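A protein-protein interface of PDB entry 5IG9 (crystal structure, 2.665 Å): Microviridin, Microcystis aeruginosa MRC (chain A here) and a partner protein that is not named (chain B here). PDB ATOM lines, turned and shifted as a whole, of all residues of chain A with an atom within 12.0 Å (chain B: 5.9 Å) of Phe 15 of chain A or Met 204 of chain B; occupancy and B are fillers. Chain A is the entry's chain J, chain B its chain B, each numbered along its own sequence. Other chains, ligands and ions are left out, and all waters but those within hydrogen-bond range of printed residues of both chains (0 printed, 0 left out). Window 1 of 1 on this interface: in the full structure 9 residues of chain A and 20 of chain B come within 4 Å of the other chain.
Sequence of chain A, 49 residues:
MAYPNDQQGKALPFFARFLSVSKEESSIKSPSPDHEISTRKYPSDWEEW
N of Phe 14 of chain A is in hydrogen-bond range of O of Gly 198 of chain B (3.0 Å).
O of Leu 143 of chain B is in hydrogen-bond range of N of Phe 206 of chain B, at 2.8 Å. O of Met 204 of chain B is in hydrogen-bond range of N of Ser 145 of chain B, 3.2 Å away. The side-chain hydroxyl (OG1) of Thr 165 of chain B sits close to the side-chain sulfur (SD) of Met 204 of chain B, 3.6 Å away.
Gly 198 of chain B touches Pro 13 of chain A (O to CA, 3.6 Å). Pro 13 of chain A touches Cys 202 of chain B. CD2 of Phe 14 of chain A touches CD2 of Leu 199 of chain B (3.6 Å). Phe 206 of chain B touches Phe 14 of chain A (CZ to CE2, 3.8 Å). Phe 15 of chain A touches Phe 171 of chain B. Phe 15 of chain A touches Val 183 of chain B (O to CG2, 3.9 Å). Phe 15 of chain A touches Cys 202 of chain B. Met 204 of chain B touches Phe 15 of chain A (SD to CA, 3.7 Å). Phe 18 of chain A touches Val 183 of chain B. Val 183 of chain B touches Leu 19 of chain A (CG2 to CD2, 3.6 Å).
Of the printed residues of chain A, Met 204 of chain B touches Phe 14 (3.6 Å) and Phe 15 (3.7 Å). No residue of chain A comes within 4 Å of Thr 144 of chain B. Thr 165 of chain B touches one residue of chain A. Printed residues of chain A within 4 Å of Met 167 of chain B: Phe 15. Val 183 of chain B touches just these residues of chain A: Phe 15 (3.9 Å), Phe 18 (3.9 Å) and Leu 19 (3.6 Å). Of chain A, only Pro 13 (3.8 Å) and Phe 15 (3.5 Å) come within 4 Å of Cys 202 of chain B. Printed residues of chain B within 4 Å of Leu 19 of chain A: Val 183 (3.6 Å). Of the printed residues of chain A, Phe 171 of chain B touches Phe 15 (3.9 Å). Of the printed residues of chain B, Phe 14 of chain A touches Gly 198, Leu 199, Met 204 and Phe 206. Printed residues of chain B within 4 Å of Phe 18 of chain A: Thr 165 and Val 183. Of the printed residues of chain B, Leu 12 of chain A touches Gly 198. Arg 17 of chain A touches none of the printed residues of chain B. The nearest printed residue of chain B that does not touch Leu 19 of chain A is Ile 173 of chain B (4.4 Å).
Among the printed residues, 15 pairs touch across the chains. Among the printed residues, no Asp or Glu carboxylate lies within 4 Å of a Lys or Arg side-chain nitrogen of the other chain.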
ATOM      1  N   ALA A  11      18.691  24.449   6.907  1.00  0.00           N
ATOM      2  CA  ALA A  11      17.294  24.056   6.759  1.00  0.00           C
ATOM      3  C   ALA A  11      17.189  22.572   6.426  1.00  0.00           C
ATOM      4  O   ALA A  11      17.027  22.197   5.265  1.00  0.00           O
ATOM      5  CB  ALA A  11      16.615  24.894   5.686  1.00  0.00           C
ATOM      6  N   LEU A  12      17.288  21.706   7.489  1.00  0.00           N
ATOM      7  CA  LEU A  12      17.288  20.252   7.396  1.00  0.00           C
ATOM      8  C   LEU A  12      15.964  19.670   7.878  1.00  0.00           C
ATOM      9  O   LEU A  12      15.404  20.136   8.877  1.00  0.00           O
ATOM     10  CB  LEU A  12      18.424  19.653   8.226  1.00  0.00           C
ATOM     11  CG  LEU A  12      19.860  19.919   7.769  1.00  0.00           C
ATOM     12  CD1 LEU A  12      20.841  19.323   8.765  1.00  0.00           C
ATOM     13  CD2 LEU A  12      20.095  19.354   6.377  1.00  0.00           C
ATOM     14  N   PRO A  13      15.450  18.661   7.184  1.00  0.00           N
ATOM     15  CA  PRO A  13      14.256  17.960   7.664  1.00  0.00           C
ATOM     16  C   PRO A  13      14.597  16.944   8.744  1.00  0.00           C
ATOM     17  O   PRO A  13      15.756  16.576   8.957  1.00  0.00           O
ATOM     18  CB  PRO A  13      13.724  17.270   6.403  1.00  0.00           C
ATOM     19  CG  PRO A  13      14.938  17.050   5.574  1.00  0.00           C
ATOM     20  CD  PRO A  13      15.864  18.202   5.847  1.00  0.00           C
ATOM     21  N   PHE A  14      13.548  16.484   9.429  1.00  0.00           N
ATOM     22  CA  PHE A  14      13.743  15.630  10.596  1.00  0.00           C
ATOM     23  C   PHE A  14      14.242  14.243  10.218  1.00  0.00           C
ATOM     24  O   PHE A  14      14.967  13.616  11.001  1.00  0.00           O
ATOM     25  CB  PHE A  14      12.444  15.518  11.394  1.00  0.00           C
ATOM     26  CG  PHE A  14      12.552  14.640  12.608  1.00  0.00           C
ATOM     27  CD1 PHE A  14      13.394  14.982  13.653  1.00  0.00           C
ATOM     28  CD2 PHE A  14      11.802  13.481  12.710  1.00  0.00           C
ATOM     29  CE1 PHE A  14      13.491  14.178  14.773  1.00  0.00           C
ATOM     30  CE2 PHE A  14      11.893  12.676  13.829  1.00  0.00           C
ATOM     31  CZ  PHE A  14      12.741  13.025  14.861  1.00  0.00           C
ATOM     32  N   PHE A  15      13.876  13.742   9.038  1.00  0.00           N
ATOM     33  CA  PHE A  15      14.309  12.400   8.673  1.00  0.00           C
ATOM     34  C   PHE A  15      15.803  12.321   8.380  1.00  0.00           C
ATOM     35  O   PHE A  15      16.315  11.213   8.189  1.00  0.00           O
ATOM     36  CB  PHE A  15      13.506  11.881   7.472  1.00  0.00           C
ATOM     37  CG  PHE A  15      13.856  12.534   6.160  1.00  0.00           C
ATOM     38  CD1 PHE A  15      14.886  12.038   5.374  1.00  0.00           C
ATOM     39  CD2 PHE A  15      13.133  13.619   5.696  1.00  0.00           C
ATOM     40  CE1 PHE A  15      15.203  12.627   4.167  1.00  0.00           C
ATOM     41  CE2 PHE A  15      13.443  14.209   4.484  1.00  0.00           C
ATOM     42  CZ  PHE A  15      14.480  13.714   3.721  1.00  0.00           C
ATOM     43  N   ALA A  16      16.509  13.454   8.341  1.00  0.00           N
ATOM     44  CA  ALA A  16      17.947  13.416   8.096  1.00  0.00           C
ATOM     45  C   ALA A  16      18.695  12.770   9.256  1.00  0.00           C
ATOM     46  O   ALA A  16      19.776  12.201   9.061  1.00  0.00           O
ATOM     47  CB  ALA A  16      18.474  14.828   7.835  1.00  0.00           C
ATOM     48  N   ARG A  17      18.130  12.831  10.463  1.00  0.00           N
ATOM     49  CA  ARG A  17      18.755  12.241  11.640  1.00  0.00           C
ATOM     50  C   ARG A  17      18.783  10.719  11.602  1.00  0.00           C
ATOM     51  O   ARG A  17      19.499  10.111  12.405  1.00  0.00           O
ATOM     52  CB  ARG A  17      18.019  12.699  12.900  1.00  0.00           C
ATOM     53  CG  ARG A  17      17.909  14.205  13.046  1.00  0.00           C
ATOM     54  CD  ARG A  17      17.150  14.570  14.309  1.00  0.00           C
ATOM     55  NE  ARG A  17      17.687  13.877  15.476  1.00  0.00           N
ATOM     56  CZ  ARG A  17      18.760  14.274  16.153  1.00  0.00           C
ATOM     57  NH1 ARG A  17      19.416  15.363  15.778  1.00  0.00           N
ATOM     58  NH2 ARG A  17      19.180  13.578  17.201  1.00  0.00           N
ATOM     59  N   PHE A  18      18.030  10.090  10.699  1.00  0.00           N
ATOM     60  CA  PHE A  18      17.880   8.640  10.680  1.00  0.00           C
ATOM     61  C   PHE A  18      18.403   8.023   9.388  1.00  0.00           C
ATOM     62  O   PHE A  18      18.048   6.886   9.058  1.00  0.00           O
ATOM     63  CB  PHE A  18      16.414   8.258  10.897  1.00  0.00           C
ATOM     64  CG  PHE A  18      15.791   8.902  12.104  1.00  0.00           C
ATOM     65  CD1 PHE A  18      15.232  10.167  12.020  1.00  0.00           C
ATOM     66  CD2 PHE A  18      15.763   8.243  13.321  1.00  0.00           C
ATOM     67  CE1 PHE A  18      14.661  10.763  13.124  1.00  0.00           C
ATOM     68  CE2 PHE A  18      15.192   8.834  14.430  1.00  0.00           C
ATOM     69  CZ  PHE A  18      14.639  10.095  14.331  1.00  0.00           C
ATOM     70  N   LEU A  19      19.241   8.747   8.652  1.00  0.00           N
ATOM     71  CA  LEU A  19      19.788   8.251   7.395  1.00  0.00           C
ATOM     72  C   LEU A  19      20.934   7.286   7.676  1.00  0.00           C
ATOM     73  O   LEU A  19      21.964   7.679   8.234  1.00  0.00           O
ATOM     74  CB  LEU A  19      20.259   9.413   6.524  1.00  0.00           C
ATOM     75  CG  LEU A  19      19.192  10.136   5.700  1.00  0.00           C
ATOM     76  CD1 LEU A  19      19.692  11.495   5.243  1.00  0.00           C
ATOM     77  CD2 LEU A  19      18.794   9.288   4.505  1.00  0.00           C
ATOM     78  N   SER A  20      20.755   6.028   7.292  1.00  0.00           N
ATOM     79  CA  SER A  20      21.774   5.005   7.440  1.00  0.00           C
ATOM     80  C   SER A  20      22.479   4.794   6.101  1.00  0.00           C
ATOM     81  O   SER A  20      22.299   5.560   5.152  1.00  0.00           O
ATOM     82  CB  SER A  20      21.144   3.715   7.971  1.00  0.00           C
ATOM     83  OG  SER A  20      20.004   3.357   7.209  1.00  0.00           O
ATOM     84  N   VAL A  21      23.295   3.745   6.019  1.00  0.00           N
ATOM     85  CA  VAL A  21      24.034   3.409   4.807  1.00  0.00           C
ATOM     86  C   VAL A  21      23.512   2.077   4.283  1.00  0.00           C
ATOM     87  O   VAL A  21      23.455   1.090   5.026  1.00  0.00           O
ATOM     88  CB  VAL A  21      25.551   3.346   5.065  1.00  0.00           C
ATOM     89  CG1 VAL A  21      26.285   2.891   3.815  1.00  0.00           C
ATOM     90  CG2 VAL A  21      26.065   4.705   5.524  1.00  0.00           C
ATOM     91  N   LEU B 143       1.336   6.892  14.406  1.00  0.00           N
ATOM     92  CA  LEU B 143       1.124   8.334  14.341  1.00  0.00           C
ATOM     93  C   LEU B 143       1.942   8.891  13.187  1.00  0.00           C
ATOM     94  O   LEU B 143       3.176   8.882  13.237  1.00  0.00           O
ATOM     95  CB  LEU B 143       1.510   9.021  15.650  1.00  0.00           C
ATOM     96  CG  LEU B 143       1.588  10.547  15.562  1.00  0.00           C
ATOM     97  CD1 LEU B 143       0.221  11.155  15.280  1.00  0.00           C
ATOM     98  CD2 LEU B 143       2.187  11.130  16.829  1.00  0.00           C
ATOM     99  N   THR B 144       1.260   9.362  12.147  1.00  0.00           N
ATOM    100  CA  THR B 144       1.877  10.182  11.114  1.00  0.00           C
ATOM    101  C   THR B 144       1.644  11.642  11.472  1.00  0.00           C
ATOM    102  O   THR B 144       0.496  12.060  11.662  1.00  0.00           O
ATOM    103  CB  THR B 144       1.298   9.873   9.733  1.00  0.00           C
ATOM    104  OG1 THR B 144       1.670   8.547   9.338  1.00  0.00           O
ATOM    105  CG2 THR B 144       1.818  10.869   8.706  1.00  0.00           C
ATOM    106  N   SER B 145       2.725  12.411  11.571  1.00  0.00           N
ATOM    107  CA  SER B 145       2.596  13.756  12.109  1.00  0.00           C
ATOM    108  C   SER B 145       3.798  14.604  11.721  1.00  0.00           C
ATOM    109  O   SER B 145       4.898  14.090  11.502  1.00  0.00           O
ATOM    110  CB  SER B 145       2.451  13.721  13.636  1.00  0.00           C
ATOM    111  OG  SER B 145       2.471  15.027  14.179  1.00  0.00           O
ATOM    112  N   ASN B 146       3.559  15.914  11.630  1.00  0.00           N
ATOM    113  CA  ASN B 146       4.607  16.925  11.580  1.00  0.00           C
ATOM    114  C   ASN B 146       4.605  17.786  12.839  1.00  0.00           C
ATOM    115  O   ASN B 146       5.122  18.906  12.827  1.00  0.00           O
ATOM    116  CB  ASN B 146       4.450  17.804  10.337  1.00  0.00           C
ATOM    117  CG  ASN B 146       3.197  18.658  10.383  1.00  0.00           C
ATOM    118  OD1 ASN B 146       2.126  18.192  10.767  1.00  0.00           O
ATOM    119  ND2 ASN B 146       3.329  19.924   9.999  1.00  0.00           N
ATOM    120  N   THR B 165      10.447   4.966  14.105  1.00  0.00           N
ATOM    121  CA  THR B 165      10.005   5.893  13.078  1.00  0.00           C
ATOM    122  C   THR B 165      10.344   5.324  11.709  1.00  0.00           C
ATOM    123  O   THR B 165      11.288   4.543  11.560  1.00  0.00           O
ATOM    124  CB  THR B 165      10.639   7.282  13.249  1.00  0.00           C
ATOM    125  OG1 THR B 165       9.971   8.214  12.396  1.00  0.00           O
ATOM    126  CG2 THR B 165      12.111   7.251  12.887  1.00  0.00           C
ATOM    127  N   LYS B 166       9.555   5.718  10.711  1.00  0.00           N
ATOM    128  CA  LYS B 166       9.746   5.217   9.359  1.00  0.00           C
ATOM    129  C   LYS B 166       9.145   6.209   8.375  1.00  0.00           C
ATOM    130  O   LYS B 166       8.298   7.033   8.728  1.00  0.00           O
ATOM    131  CB  LYS B 166       9.126   3.832   9.180  1.00  0.00           C
ATOM    132  CG  LYS B 166       7.608   3.811   9.264  1.00  0.00           C
ATOM    133  CD  LYS B 166       7.089   2.380   9.225  1.00  0.00           C
ATOM    134  CE  LYS B 166       5.573   2.315   9.339  1.00  0.00           C
ATOM    135  NZ  LYS B 166       4.884   2.788   8.106  1.00  0.00           N
ATOM    136  N   MET B 167       9.600   6.116   7.129  1.00  0.00           N
ATOM    137  CA  MET B 167       9.100   6.947   6.045  1.00  0.00           C
ATOM    138  C   MET B 167       8.056   6.173   5.254  1.00  0.00           C
ATOM    139  O   MET B 167       8.219   4.976   4.999  1.00  0.00           O
ATOM    140  CB  MET B 167      10.239   7.388   5.122  1.00  0.00           C
ATOM    141  CG  MET B 167      11.245   8.330   5.766  1.00  0.00           C
ATOM    142  SD  MET B 167      10.558   9.947   6.179  1.00  0.00           S
ATOM    143  CE  MET B 167      10.663  10.792   4.602  1.00  0.00           C
ATOM    144  N   PHE B 171      12.837   6.082  -1.221  1.00  0.00           N
ATOM    145  CA  PHE B 171      13.781   6.992  -1.860  1.00  0.00           C
ATOM    146  C   PHE B 171      15.186   6.618  -1.403  1.00  0.00           C
ATOM    147  O   PHE B 171      15.388   5.649  -0.665  1.00  0.00           O
ATOM    148  CB  PHE B 171      13.454   8.452  -1.537  1.00  0.00           C
ATOM    149  CG  PHE B 171      13.488   8.769  -0.073  1.00  0.00           C
ATOM    150  CD1 PHE B 171      14.670   9.156   0.539  1.00  0.00           C
ATOM    151  CD2 PHE B 171      12.341   8.679   0.697  1.00  0.00           C
ATOM    152  CE1 PHE B 171      14.707   9.444   1.886  1.00  0.00           C
ATOM    153  CE2 PHE B 171      12.372   8.967   2.045  1.00  0.00           C
ATOM    154  CZ  PHE B 171      13.557   9.352   2.641  1.00  0.00           C
ATOM    155  N   ILE B 173      19.020   8.998  -0.655  1.00  0.00           N
ATOM    156  CA  ILE B 173      19.850  10.193  -0.751  1.00  0.00           C
ATOM    157  C   ILE B 173      21.264   9.754  -1.099  1.00  0.00           C
ATOM    158  O   ILE B 173      21.853   8.912  -0.410  1.00  0.00           O
ATOM    159  CB  ILE B 173      19.820  11.015   0.549  1.00  0.00           C
ATOM    160  CG1 ILE B 173      18.689  12.043   0.497  1.00  0.00           C
ATOM    161  CG2 ILE B 173      21.149  11.727   0.780  1.00  0.00           C
ATOM    162  CD1 ILE B 173      17.303  11.448   0.510  1.00  0.00           C
ATOM    163  N   VAL B 183      16.575   5.482   4.751  1.00  0.00           N
ATOM    164  CA  VAL B 183      15.974   5.552   6.080  1.00  0.00           C
ATOM    165  C   VAL B 183      15.268   4.225   6.337  1.00  0.00           C
ATOM    166  O   VAL B 183      14.155   3.996   5.861  1.00  0.00           O
ATOM    167  CB  VAL B 183      15.010   6.732   6.211  1.00  0.00           C
ATOM    168  CG1 VAL B 183      14.313   6.702   7.570  1.00  0.00           C
ATOM    169  CG2 VAL B 183      15.738   8.048   6.021  1.00  0.00           C
ATOM    170  N   GLY B 198      12.799  19.690  13.099  1.00  0.00           N
ATOM    171  CA  GLY B 198      12.823  19.430  11.670  1.00  0.00           C
ATOM    172  C   GLY B 198      11.560  18.812  11.109  1.00  0.00           C
ATOM    173  O   GLY B 198      11.502  18.558   9.903  1.00  0.00           O
ATOM    174  N   LEU B 199      10.554  18.551  11.949  1.00  0.00           N
ATOM    175  CA  LEU B 199       9.302  17.983  11.463  1.00  0.00           C
ATOM    176  C   LEU B 199       8.512  18.967  10.612  1.00  0.00           C
ATOM    177  O   LEU B 199       7.672  18.540   9.813  1.00  0.00           O
ATOM    178  CB  LEU B 199       8.450  17.506  12.639  1.00  0.00           C
ATOM    179  CG  LEU B 199       8.803  16.143  13.239  1.00  0.00           C
ATOM    180  CD1 LEU B 199       7.968  15.873  14.478  1.00  0.00           C
ATOM    181  CD2 LEU B 199       8.607  15.042  12.212  1.00  0.00           C
ATOM    182  N   CYS B 202       9.398  18.004   6.956  1.00  0.00           N
ATOM    183  CA  CYS B 202       8.997  16.698   6.454  1.00  0.00           C
ATOM    184  C   CYS B 202       8.407  15.880   7.594  1.00  0.00           C
ATOM    185  O   CYS B 202       9.054  15.702   8.633  1.00  0.00           O
ATOM    186  CB  CYS B 202      10.182  15.958   5.827  1.00  0.00           C
ATOM    187  SG  CYS B 202       9.778  14.337   5.127  1.00  0.00           S
ATOM    188  N   PRO B 203       7.189  15.371   7.446  1.00  0.00           N
ATOM    189  CA  PRO B 203       6.615  14.519   8.488  1.00  0.00           C
ATOM    190  C   PRO B 203       7.255  13.139   8.470  1.00  0.00           C
ATOM    191  O   PRO B 203       7.963  12.755   7.538  1.00  0.00           O
ATOM    192  CB  PRO B 203       5.135  14.456   8.110  1.00  0.00           C
ATOM    193  CG  PRO B 203       5.149  14.573   6.633  1.00  0.00           C
ATOM    194  CD  PRO B 203       6.277  15.522   6.301  1.00  0.00           C
ATOM    195  N   MET B 204       7.001  12.390   9.540  1.00  0.00           N
ATOM    196  CA  MET B 204       7.423  11.002   9.626  1.00  0.00           C
ATOM    197  C   MET B 204       6.294  10.185  10.230  1.00  0.00           C
ATOM    198  O   MET B 204       5.330  10.724  10.780  1.00  0.00           O
ATOM    199  CB  MET B 204       8.708  10.838  10.456  1.00  0.00           C
ATOM    200  CG  MET B 204       9.939  11.493   9.847  1.00  0.00           C
ATOM    201  SD  MET B 204      11.488  10.754  10.406  1.00  0.00           S
ATOM    202  CE  MET B 204      11.392   9.136   9.642  1.00  0.00           C
ATOM    203  N   THR B 205       6.419   8.868  10.120  1.00  0.00           N
ATOM    204  CA  THR B 205       5.433   7.934  10.646  1.00  0.00           C
ATOM    205  C   THR B 205       6.053   7.186  11.819  1.00  0.00           C
ATOM    206  O   THR B 205       7.026   6.445  11.645  1.00  0.00           O
ATOM    207  CB  THR B 205       4.969   6.962   9.562  1.00  0.00           C
ATOM    208  OG1 THR B 205       4.419   7.703   8.465  1.00  0.00           O
ATOM    209  CG2 THR B 205       3.906   6.029  10.105  1.00  0.00           C
ATOM    210  N   PHE B 206       5.498   7.390  13.010  1.00  0.00           N
ATOM    211  CA  PHE B 206       5.979   6.757  14.228  1.00  0.00           C
ATOM    212  C   PHE B 206       5.050   5.613  14.614  1.00  0.00           C
ATOM    213  O   PHE B 206       3.839   5.675  14.386  1.00  0.00           O
ATOM    214  CB  PHE B 206       6.072   7.771  15.373  1.00  0.00           C
ATOM    215  CG  PHE B 206       6.904   8.977  15.044  1.00  0.00           C
ATOM    216  CD1 PHE B 206       6.334  10.081  14.431  1.00  0.00           C
ATOM    217  CD2 PHE B 206       8.254   9.004  15.339  1.00  0.00           C
ATOM    218  CE1 PHE B 206       7.099  11.190  14.125  1.00  0.00           C
ATOM    219  CE2 PHE B 206       9.024  10.108  15.036  1.00  0.00           C
ATOM    220  CZ  PHE B 206       8.445  11.203  14.428  1.00  0.00           C
